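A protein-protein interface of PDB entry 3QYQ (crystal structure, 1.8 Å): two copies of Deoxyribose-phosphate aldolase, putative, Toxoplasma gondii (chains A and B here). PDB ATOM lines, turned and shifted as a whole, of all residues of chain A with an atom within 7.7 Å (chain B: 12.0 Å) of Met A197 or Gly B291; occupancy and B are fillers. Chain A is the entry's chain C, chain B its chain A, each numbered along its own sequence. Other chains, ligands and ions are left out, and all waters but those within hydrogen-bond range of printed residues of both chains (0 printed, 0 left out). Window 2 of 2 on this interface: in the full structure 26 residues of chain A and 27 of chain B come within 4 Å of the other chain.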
ATOM      1  N   HIS A 194     -27.067  22.465  -0.581  1.00  0.00           N
ATOM      2  CA  HIS A 194     -26.713  21.475   0.428  1.00  0.00           C
ATOM      3  C   HIS A 194     -25.461  21.951   1.167  1.00  0.00           C
ATOM      4  O   HIS A 194     -25.145  23.146   1.159  1.00  0.00           O
ATOM      5  CB  HIS A 194     -26.527  20.125  -0.266  1.00  0.00           C
ATOM      6  CG  HIS A 194     -27.688  19.760  -1.137  1.00  0.00           C
ATOM      7  ND1 HIS A 194     -28.756  19.014  -0.687  1.00  0.00           N
ATOM      8  CD2 HIS A 194     -27.988  20.117  -2.410  1.00  0.00           C
ATOM      9  CE1 HIS A 194     -29.646  18.895  -1.657  1.00  0.00           C
ATOM     10  NE2 HIS A 194     -29.203  19.554  -2.714  1.00  0.00           N
ATOM     11  N   ALA A 195     -24.743  21.049   1.816  1.00  0.00           N
ATOM     12  CA  ALA A 195     -23.545  21.473   2.540  1.00  0.00           C
ATOM     13  C   ALA A 195     -22.472  22.096   1.629  1.00  0.00           C
ATOM     14  O   ALA A 195     -22.360  21.762   0.457  1.00  0.00           O
ATOM     15  CB  ALA A 195     -22.950  20.292   3.324  1.00  0.00           C
ATOM     16  N   THR A 196     -21.745  23.054   2.190  1.00  0.00           N
ATOM     17  CA  THR A 196     -20.627  23.724   1.538  1.00  0.00           C
ATOM     18  C   THR A 196     -19.602  23.720   2.655  1.00  0.00           C
ATOM     19  O   THR A 196     -19.980  23.624   3.834  1.00  0.00           O
ATOM     20  CB  THR A 196     -20.900  25.188   1.097  1.00  0.00           C
ATOM     21  OG1 THR A 196     -21.272  25.977   2.235  1.00  0.00           O
ATOM     22  CG2 THR A 196     -22.007  25.261   0.047  1.00  0.00           C
ATOM     23  N   MET A 197     -18.322  23.810   2.316  1.00  0.00           N
ATOM     24  CA  MET A 197     -17.273  23.840   3.325  1.00  0.00           C
ATOM     25  C   MET A 197     -17.543  25.013   4.268  1.00  0.00           C
ATOM     26  O   MET A 197     -17.383  24.912   5.493  1.00  0.00           O
ATOM     27  CB  MET A 197     -15.911  23.979   2.646  1.00  0.00           C
ATOM     28  CG  MET A 197     -14.706  24.008   3.568  1.00  0.00           C
ATOM     29  SD  MET A 197     -13.153  24.136   2.618  1.00  0.00           S
ATOM     30  CE  MET A 197     -11.928  24.007   3.925  1.00  0.00           C
ATOM     31  N   PHE A 198     -17.993  26.119   3.691  1.00  0.00           N
ATOM     32  CA  PHE A 198     -18.310  27.319   4.459  1.00  0.00           C
ATOM     33  C   PHE A 198     -19.365  27.081   5.550  1.00  0.00           C
ATOM     34  O   PHE A 198     -19.157  27.452   6.709  1.00  0.00           O
ATOM     35  CB  PHE A 198     -18.773  28.404   3.484  1.00  0.00           C
ATOM     36  CG  PHE A 198     -19.266  29.652   4.139  1.00  0.00           C
ATOM     37  CD1 PHE A 198     -18.382  30.641   4.531  1.00  0.00           C
ATOM     38  CD2 PHE A 198     -20.626  29.861   4.314  1.00  0.00           C
ATOM     39  CE1 PHE A 198     -18.841  31.804   5.126  1.00  0.00           C
ATOM     40  CE2 PHE A 198     -21.091  31.022   4.901  1.00  0.00           C
ATOM     41  CZ  PHE A 198     -20.194  31.994   5.305  1.00  0.00           C
ATOM     42  N   THR A 199     -20.478  26.457   5.180  1.00  0.00           N
ATOM     43  CA  THR A 199     -21.554  26.177   6.135  1.00  0.00           C
ATOM     44  C   THR A 199     -21.142  25.150   7.195  1.00  0.00           C
ATOM     45  O   THR A 199     -21.483  25.300   8.365  1.00  0.00           O
ATOM     46  CB  THR A 199     -22.840  25.711   5.429  1.00  0.00           C
ATOM     47  OG1 THR A 199     -23.336  26.766   4.594  1.00  0.00           O
ATOM     48  CG2 THR A 199     -23.916  25.344   6.453  1.00  0.00           C
ATOM     49  N   VAL A 200     -20.426  24.105   6.787  1.00  0.00           N
ATOM     50  CA  VAL A 200     -19.964  23.075   7.740  1.00  0.00           C
ATOM     51  C   VAL A 200     -19.013  23.724   8.745  1.00  0.00           C
ATOM     52  O   VAL A 200     -19.040  23.418   9.935  1.00  0.00           O
ATOM     53  CB  VAL A 200     -19.288  21.882   7.047  1.00  0.00           C
ATOM     54  CG1 VAL A 200     -18.616  20.957   8.072  1.00  0.00           C
ATOM     55  CG2 VAL A 200     -20.314  21.127   6.192  1.00  0.00           C
ATOM     56  N   HIS A 201     -18.185  24.645   8.263  1.00  0.00           N
ATOM     57  CA  HIS A 201     -17.244  25.353   9.109  1.00  0.00           C
ATOM     58  C   HIS A 201     -17.970  26.182  10.155  1.00  0.00           C
ATOM     59  O   HIS A 201     -17.606  26.132  11.337  1.00  0.00           O
ATOM     60  CB  HIS A 201     -16.322  26.239   8.262  1.00  0.00           C
ATOM     61  CG  HIS A 201     -15.380  27.084   9.062  1.00  0.00           C
ATOM     62  ND1 HIS A 201     -14.271  26.567   9.701  1.00  0.00           N
ATOM     63  CD2 HIS A 201     -15.342  28.422   9.272  1.00  0.00           C
ATOM     64  CE1 HIS A 201     -13.616  27.544  10.303  1.00  0.00           C
ATOM     65  NE2 HIS A 201     -14.244  28.680  10.058  1.00  0.00           N
ATOM     66  N   LEU A 202     -18.981  26.936   9.732  1.00  0.00           N
ATOM     67  CA  LEU A 202     -19.755  27.766  10.670  1.00  0.00           C
ATOM     68  C   LEU A 202     -20.491  26.930  11.712  1.00  0.00           C
ATOM     69  O   LEU A 202     -20.553  27.306  12.883  1.00  0.00           O
ATOM     70  CB  LEU A 202     -20.741  28.675   9.942  1.00  0.00           C
ATOM     71  CG  LEU A 202     -20.115  29.765   9.062  1.00  0.00           C
ATOM     72  CD1 LEU A 202     -21.173  30.476   8.222  1.00  0.00           C
ATOM     73  CD2 LEU A 202     -19.310  30.756   9.889  1.00  0.00           C
ATOM     74  N   ILE A 203     -21.077  25.819  11.277  1.00  0.00           N
ATOM     75  CA  ILE A 203     -21.787  24.921  12.183  1.00  0.00           C
ATOM     76  C   ILE A 203     -20.819  24.295  13.194  1.00  0.00           C
ATOM     77  O   ILE A 203     -21.124  24.211  14.402  1.00  0.00           O
ATOM     78  CB  ILE A 203     -22.559  23.855  11.401  1.00  0.00           C
ATOM     79  CG1 ILE A 203     -23.733  24.523  10.672  1.00  0.00           C
ATOM     80  CG2 ILE A 203     -23.067  22.790  12.343  1.00  0.00           C
ATOM     81  CD1 ILE A 203     -24.477  23.623   9.683  1.00  0.00           C
ATOM     82  N   SER A 204     -19.647  23.880  12.723  1.00  0.00           N
ATOM     83  CA  SER A 204     -18.631  23.295  13.604  1.00  0.00           C
ATOM     84  C   SER A 204     -18.178  24.291  14.667  1.00  0.00           C
ATOM     85  O   SER A 204     -18.060  23.939  15.856  1.00  0.00           O
ATOM     86  CB  SER A 204     -17.422  22.792  12.816  1.00  0.00           C
ATOM     87  OG  SER A 204     -17.771  21.712  11.976  1.00  0.00           O
ATOM     88  N   GLU A 246     -16.471  14.427  -3.483  1.00  0.00           N
ATOM     89  CA  GLU A 246     -16.856  15.588  -2.708  1.00  0.00           C
ATOM     90  C   GLU A 246     -17.236  15.193  -1.274  1.00  0.00           C
ATOM     91  O   GLU A 246     -16.918  15.900  -0.298  1.00  0.00           O
ATOM     92  CB  GLU A 246     -17.997  16.290  -3.441  1.00  0.00           C
ATOM     93  CG  GLU A 246     -18.535  17.485  -2.753  1.00  0.00           C
ATOM     94  CD  GLU A 246     -19.544  18.229  -3.612  1.00  0.00           C
ATOM     95  OE1 GLU A 246     -19.667  17.900  -4.814  1.00  0.00           O
ATOM     96  OE2 GLU A 246     -20.194  19.155  -3.086  1.00  0.00           O
ATOM     97  N   ASP A 249     -14.220  14.771   0.782  1.00  0.00           N
ATOM     98  CA  ASP A 249     -13.629  16.043   1.141  1.00  0.00           C
ATOM     99  C   ASP A 249     -14.325  16.550   2.420  1.00  0.00           C
ATOM    100  O   ASP A 249     -13.667  17.110   3.293  1.00  0.00           O
ATOM    101  CB  ASP A 249     -13.768  17.046   0.010  1.00  0.00           C
ATOM    102  CG  ASP A 249     -12.879  18.266   0.192  1.00  0.00           C
ATOM    103  OD1 ASP A 249     -11.693  18.132   0.595  1.00  0.00           O
ATOM    104  OD2 ASP A 249     -13.344  19.366  -0.162  1.00  0.00           O
ATOM    105  N   PHE A 250     -15.648  16.373   2.528  1.00  0.00           N
ATOM    106  CA  PHE A 250     -16.359  16.792   3.752  1.00  0.00           C
ATOM    107  C   PHE A 250     -15.920  15.938   4.928  1.00  0.00           C
ATOM    108  O   PHE A 250     -15.821  16.417   6.046  1.00  0.00           O
ATOM    109  CB  PHE A 250     -17.877  16.718   3.643  1.00  0.00           C
ATOM    110  CG  PHE A 250     -18.481  17.813   2.839  1.00  0.00           C
ATOM    111  CD1 PHE A 250     -18.534  19.096   3.361  1.00  0.00           C
ATOM    112  CD2 PHE A 250     -19.066  17.568   1.626  1.00  0.00           C
ATOM    113  CE1 PHE A 250     -19.123  20.114   2.658  1.00  0.00           C
ATOM    114  CE2 PHE A 250     -19.670  18.593   0.915  1.00  0.00           C
ATOM    115  CZ  PHE A 250     -19.687  19.863   1.431  1.00  0.00           C
ATOM    116  N   GLN A 253     -12.890  17.448   6.158  1.00  0.00           N
ATOM    117  CA  GLN A 253     -13.174  18.702   6.845  1.00  0.00           C
ATOM    118  C   GLN A 253     -13.639  18.418   8.275  1.00  0.00           C
ATOM    119  O   GLN A 253     -13.205  19.075   9.213  1.00  0.00           O
ATOM    120  CB  GLN A 253     -14.219  19.503   6.073  1.00  0.00           C
ATOM    121  CG  GLN A 253     -13.734  19.880   4.684  1.00  0.00           C
ATOM    122  CD  GLN A 253     -14.776  20.592   3.865  1.00  0.00           C
ATOM    123  OE1 GLN A 253     -15.838  20.960   4.369  1.00  0.00           O
ATOM    124  NE2 GLN A 253     -14.474  20.808   2.587  1.00  0.00           N
ATOM    125  N   PHE A 256     -10.642  17.379  10.373  1.00  0.00           N
ATOM    126  CA  PHE A 256      -9.790  18.525  10.661  1.00  0.00           C
ATOM    127  C   PHE A 256     -10.405  19.459  11.696  1.00  0.00           C
ATOM    128  O   PHE A 256      -9.732  19.856  12.641  1.00  0.00           O
ATOM    129  CB  PHE A 256      -9.448  19.320   9.388  1.00  0.00           C
ATOM    130  CG  PHE A 256      -8.517  20.480   9.640  1.00  0.00           C
ATOM    131  CD1 PHE A 256      -7.162  20.261   9.811  1.00  0.00           C
ATOM    132  CD2 PHE A 256      -8.986  21.773   9.680  1.00  0.00           C
ATOM    133  CE1 PHE A 256      -6.299  21.306  10.048  1.00  0.00           C
ATOM    134  CE2 PHE A 256      -8.124  22.825   9.910  1.00  0.00           C
ATOM    135  CZ  PHE A 256      -6.777  22.587  10.099  1.00  0.00           C
ATOM    136  N   GLU A 257     -11.674  19.795  11.509  1.00  0.00           N
ATOM    137  CA  GLU A 257     -12.391  20.698  12.413  1.00  0.00           C
ATOM    138  C   GLU A 257     -12.705  20.159  13.788  1.00  0.00           C
ATOM    139  O   GLU A 257     -12.532  20.858  14.807  1.00  0.00           O
ATOM    140  CB  GLU A 257     -13.765  21.036  11.806  1.00  0.00           C
ATOM    141  CG  GLU A 257     -13.766  21.911  10.556  1.00  0.00           C
ATOM    142  CD  GLU A 257     -13.513  23.374  10.852  1.00  0.00           C
ATOM    143  OE1 GLU A 257     -13.426  24.153   9.880  1.00  0.00           O
ATOM    144  OE2 GLU A 257     -13.435  23.760  12.046  1.00  0.00           O
ATOM    145  N   PHE B  15     -10.183  15.686  -7.815  1.00  0.00           N
ATOM    146  CA  PHE B  15     -10.188  14.850  -6.606  1.00  0.00           C
ATOM    147  C   PHE B  15      -9.386  13.555  -6.734  1.00  0.00           C
ATOM    148  O   PHE B  15      -9.790  12.509  -6.214  1.00  0.00           O
ATOM    149  CB  PHE B  15     -11.616  14.513  -6.152  1.00  0.00           C
ATOM    150  CG  PHE B  15     -12.371  15.677  -5.586  1.00  0.00           C
ATOM    151  CD1 PHE B  15     -11.989  16.232  -4.379  1.00  0.00           C
ATOM    152  CD2 PHE B  15     -13.515  16.153  -6.203  1.00  0.00           C
ATOM    153  CE1 PHE B  15     -12.683  17.297  -3.834  1.00  0.00           C
ATOM    154  CE2 PHE B  15     -14.221  17.203  -5.655  1.00  0.00           C
ATOM    155  CZ  PHE B  15     -13.807  17.773  -4.460  1.00  0.00           C
ATOM    156  N   ILE B  18      -7.864  12.784  -2.905  1.00  0.00           N
ATOM    157  CA  ILE B  18      -8.696  12.797  -1.690  1.00  0.00           C
ATOM    158  C   ILE B  18      -8.787  11.476  -0.928  1.00  0.00           C
ATOM    159  O   ILE B  18      -8.742  11.473   0.297  1.00  0.00           O
ATOM    160  CB  ILE B  18     -10.126  13.362  -1.957  1.00  0.00           C
ATOM    161  CG1 ILE B  18     -10.833  13.717  -0.635  1.00  0.00           C
ATOM    162  CG2 ILE B  18     -10.971  12.404  -2.808  1.00  0.00           C
ATOM    163  CD1 ILE B  18     -10.126  14.755   0.195  1.00  0.00           C
ATOM    164  N   GLN B  21      -5.470  10.758   0.752  1.00  0.00           N
ATOM    165  CA  GLN B  21      -5.326  11.747   1.846  1.00  0.00           C
ATOM    166  C   GLN B  21      -6.110  11.308   3.076  1.00  0.00           C
ATOM    167  O   GLN B  21      -5.615  11.393   4.223  1.00  0.00           O
ATOM    168  CB  GLN B  21      -5.780  13.119   1.372  1.00  0.00           C
ATOM    169  CG  GLN B  21      -4.812  13.756   0.377  1.00  0.00           C
ATOM    170  CD  GLN B  21      -5.389  14.932  -0.408  1.00  0.00           C
ATOM    171  OE1 GLN B  21      -6.592  15.139  -0.455  1.00  0.00           O
ATOM    172  NE2 GLN B  21      -4.508  15.685  -1.080  1.00  0.00           N
ATOM    173  N   TYR B 284      -0.881  13.143   3.713  1.00  0.00           N
ATOM    174  CA  TYR B 284      -1.857  13.958   4.429  1.00  0.00           C
ATOM    175  C   TYR B 284      -1.665  15.458   4.274  1.00  0.00           C
ATOM    176  O   TYR B 284      -2.630  16.203   4.079  1.00  0.00           O
ATOM    177  CB  TYR B 284      -1.917  13.594   5.913  1.00  0.00           C
ATOM    178  CG  TYR B 284      -2.719  14.601   6.683  1.00  0.00           C
ATOM    179  CD1 TYR B 284      -4.082  14.737   6.471  1.00  0.00           C
ATOM    180  CD2 TYR B 284      -2.115  15.417   7.620  1.00  0.00           C
ATOM    181  CE1 TYR B 284      -4.814  15.676   7.152  1.00  0.00           C
ATOM    182  CE2 TYR B 284      -2.844  16.355   8.315  1.00  0.00           C
ATOM    183  CZ  TYR B 284      -4.192  16.478   8.082  1.00  0.00           C
ATOM    184  OH  TYR B 284      -4.916  17.420   8.794  1.00  0.00           O
ATOM    185  N   SER B 286      -0.715  17.107   1.860  1.00  0.00           N
ATOM    186  CA  SER B 286      -1.094  17.597   0.550  1.00  0.00           C
ATOM    187  C   SER B 286      -2.564  18.017   0.500  1.00  0.00           C
ATOM    188  O   SER B 286      -3.004  18.613  -0.472  1.00  0.00           O
ATOM    189  CB  SER B 286      -0.777  16.571  -0.538  1.00  0.00           C
ATOM    190  OG  SER B 286      -1.601  15.433  -0.483  1.00  0.00           O
ATOM    191  N   TRP B 287      -3.340  17.670   1.529  1.00  0.00           N
ATOM    192  CA  TRP B 287      -4.737  18.070   1.592  1.00  0.00           C
ATOM    193  C   TRP B 287      -4.777  19.518   2.093  1.00  0.00           C
ATOM    194  O   TRP B 287      -4.135  19.860   3.092  1.00  0.00           O
ATOM    195  CB  TRP B 287      -5.545  17.139   2.509  1.00  0.00           C
ATOM    196  CG  TRP B 287      -6.975  17.509   2.611  1.00  0.00           C
ATOM    197  CD1 TRP B 287      -7.960  17.284   1.683  1.00  0.00           C
ATOM    198  CD2 TRP B 287      -7.609  18.170   3.712  1.00  0.00           C
ATOM    199  NE1 TRP B 287      -9.159  17.785   2.139  1.00  0.00           N
ATOM    200  CE2 TRP B 287      -8.964  18.330   3.383  1.00  0.00           C
ATOM    201  CE3 TRP B 287      -7.151  18.647   4.951  1.00  0.00           C
ATOM    202  CZ2 TRP B 287      -9.872  18.949   4.246  1.00  0.00           C
ATOM    203  CZ3 TRP B 287      -8.062  19.252   5.812  1.00  0.00           C
ATOM    204  CH2 TRP B 287      -9.396  19.397   5.453  1.00  0.00           C
ATOM    205  N   ASP B 288      -5.533  20.362   1.407  1.00  0.00           N
ATOM    206  CA  ASP B 288      -5.644  21.779   1.771  1.00  0.00           C
ATOM    207  C   ASP B 288      -6.710  21.986   2.836  1.00  0.00           C
ATOM    208  O   ASP B 288      -7.898  21.904   2.558  1.00  0.00           O
ATOM    209  CB  ASP B 288      -6.011  22.614   0.552  1.00  0.00           C
ATOM    210  CG  ASP B 288      -6.170  24.093   0.876  1.00  0.00           C
ATOM    211  OD1 ASP B 288      -5.581  24.575   1.873  1.00  0.00           O
ATOM    212  OD2 ASP B 288      -6.872  24.785   0.104  1.00  0.00           O
ATOM    213  N   SER B 289      -6.272  22.293   4.050  1.00  0.00           N
ATOM    214  CA  SER B 289      -7.195  22.501   5.157  1.00  0.00           C
ATOM    215  C   SER B 289      -7.735  23.927   5.211  1.00  0.00           C
ATOM    216  O   SER B 289      -8.757  24.180   5.858  1.00  0.00           O
ATOM    217  CB  SER B 289      -6.500  22.181   6.475  1.00  0.00           C
ATOM    218  OG  SER B 289      -5.394  23.046   6.704  1.00  0.00           O
ATOM    219  N   VAL B 290      -7.078  24.859   4.527  1.00  0.00           N
ATOM    220  CA  VAL B 290      -7.522  26.252   4.562  1.00  0.00           C
ATOM    221  C   VAL B 290      -8.823  26.477   3.786  1.00  0.00           C
ATOM    222  O   VAL B 290      -8.963  26.059   2.637  1.00  0.00           O
ATOM    223  CB  VAL B 290      -6.437  27.216   4.023  1.00  0.00           C
ATOM    224  CG1 VAL B 290      -6.914  28.656   4.155  1.00  0.00           C
ATOM    225  CG2 VAL B 290      -5.133  27.036   4.779  1.00  0.00           C
ATOM    226  N   GLY B 291      -9.771  27.159   4.418  1.00  0.00           N
ATOM    227  CA  GLY B 291     -11.059  27.451   3.790  1.00  0.00           C
ATOM    228  C   GLY B 291     -11.274  28.940   3.603  1.00  0.00           C
ATOM    229  O   GLY B 291     -10.346  29.737   3.765  1.00  0.00           O
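Among the printed residues, pairs that only touch across the chains: Met A197 with Gly B291 (3.6 Å), Phe A256 with Ser B289 (3.7 Å), Met A197 with Ser B289 (3.7 Å), Asp A249 with Ile B18 (3.7 Å), Phe A256 with Tyr B284 (3.8 Å), Met A197 with Val B290 (3.8 Å), Phe A256 with Trp B287 (3.8 Å) and Gln A253 with Trp B287 (3.9 Å).
The side-chain carboxylate (OD1) of Asp B288 is in hydrogen-bond range of the backbone NH (N) of Val B290 (3.1 Å).
OD2 of Asp A249 lies within hydrogen-bond range of NE2 of Gln A253 (3.3 Å).
The side-chain sulfur (SD) of Met A197 lies close to the side-chain amide nitrogen (NE2) of Gln A253, at 3.6 Å.
The side-chain amide nitrogen of Gln B21 lies close to the backbone NH of Trp B287, 3.5 Å away.
The side-chain carboxylate of Asp A249 lies within hydrogen-bond range of the indole nitrogen of Trp B287 (3.0 Å).
No residue of chain B comes within 4 Å of Thr A196.
Printed residues of chain B within 4 Å of Met A197: Ser B289 (3.7 Å), Val B290 (3.8 Å) and Gly B291 (3.6 Å).
No residue of chain B comes within 4 Å of Val A200.
No residue of chain B comes within 4 Å of His A201.
Of the printed residues of chain B, Phe A256 touches Tyr B284 (3.8 Å), Trp B287 (3.8 Å) and Ser B289 (3.7 Å).
Of the printed residues of chain A, Ile B18 touches Asp A249.
Printed residues of chain A within 4 Å of Tyr B284: Phe A256 (3.8 Å).
Printed residues of chain A within 4 Å of Ser B289: Met A197 (3.7 Å) and Phe A256 (3.7 Å).
Gly B291 touches just one residue of chain A: Met A197.
The nearest residue of chain A that does not touch Gly B291 is His A201 (6.8 Å).
No position is printed for both chains.
Of the 9 pairs that touch across the chains among the printed residues, none has its exchanged pair printed and touching as well.
Printed residues of chain B that touch a printed residue of chain A: Ile B18, Tyr B284, Trp B287, Ser B289, Val B290 and Gly B291.
Hydrophobic or aromatic side chains of chain B within 4 Å of the printed part of chain A: Ile B18, Tyr B284 and Trp B287.
Hydrophobic or aromatic side chains of chain A that line the printed part of chain B: Met A197 and Phe A256.
Among the printed residues, 9 pairs touch across the chains.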
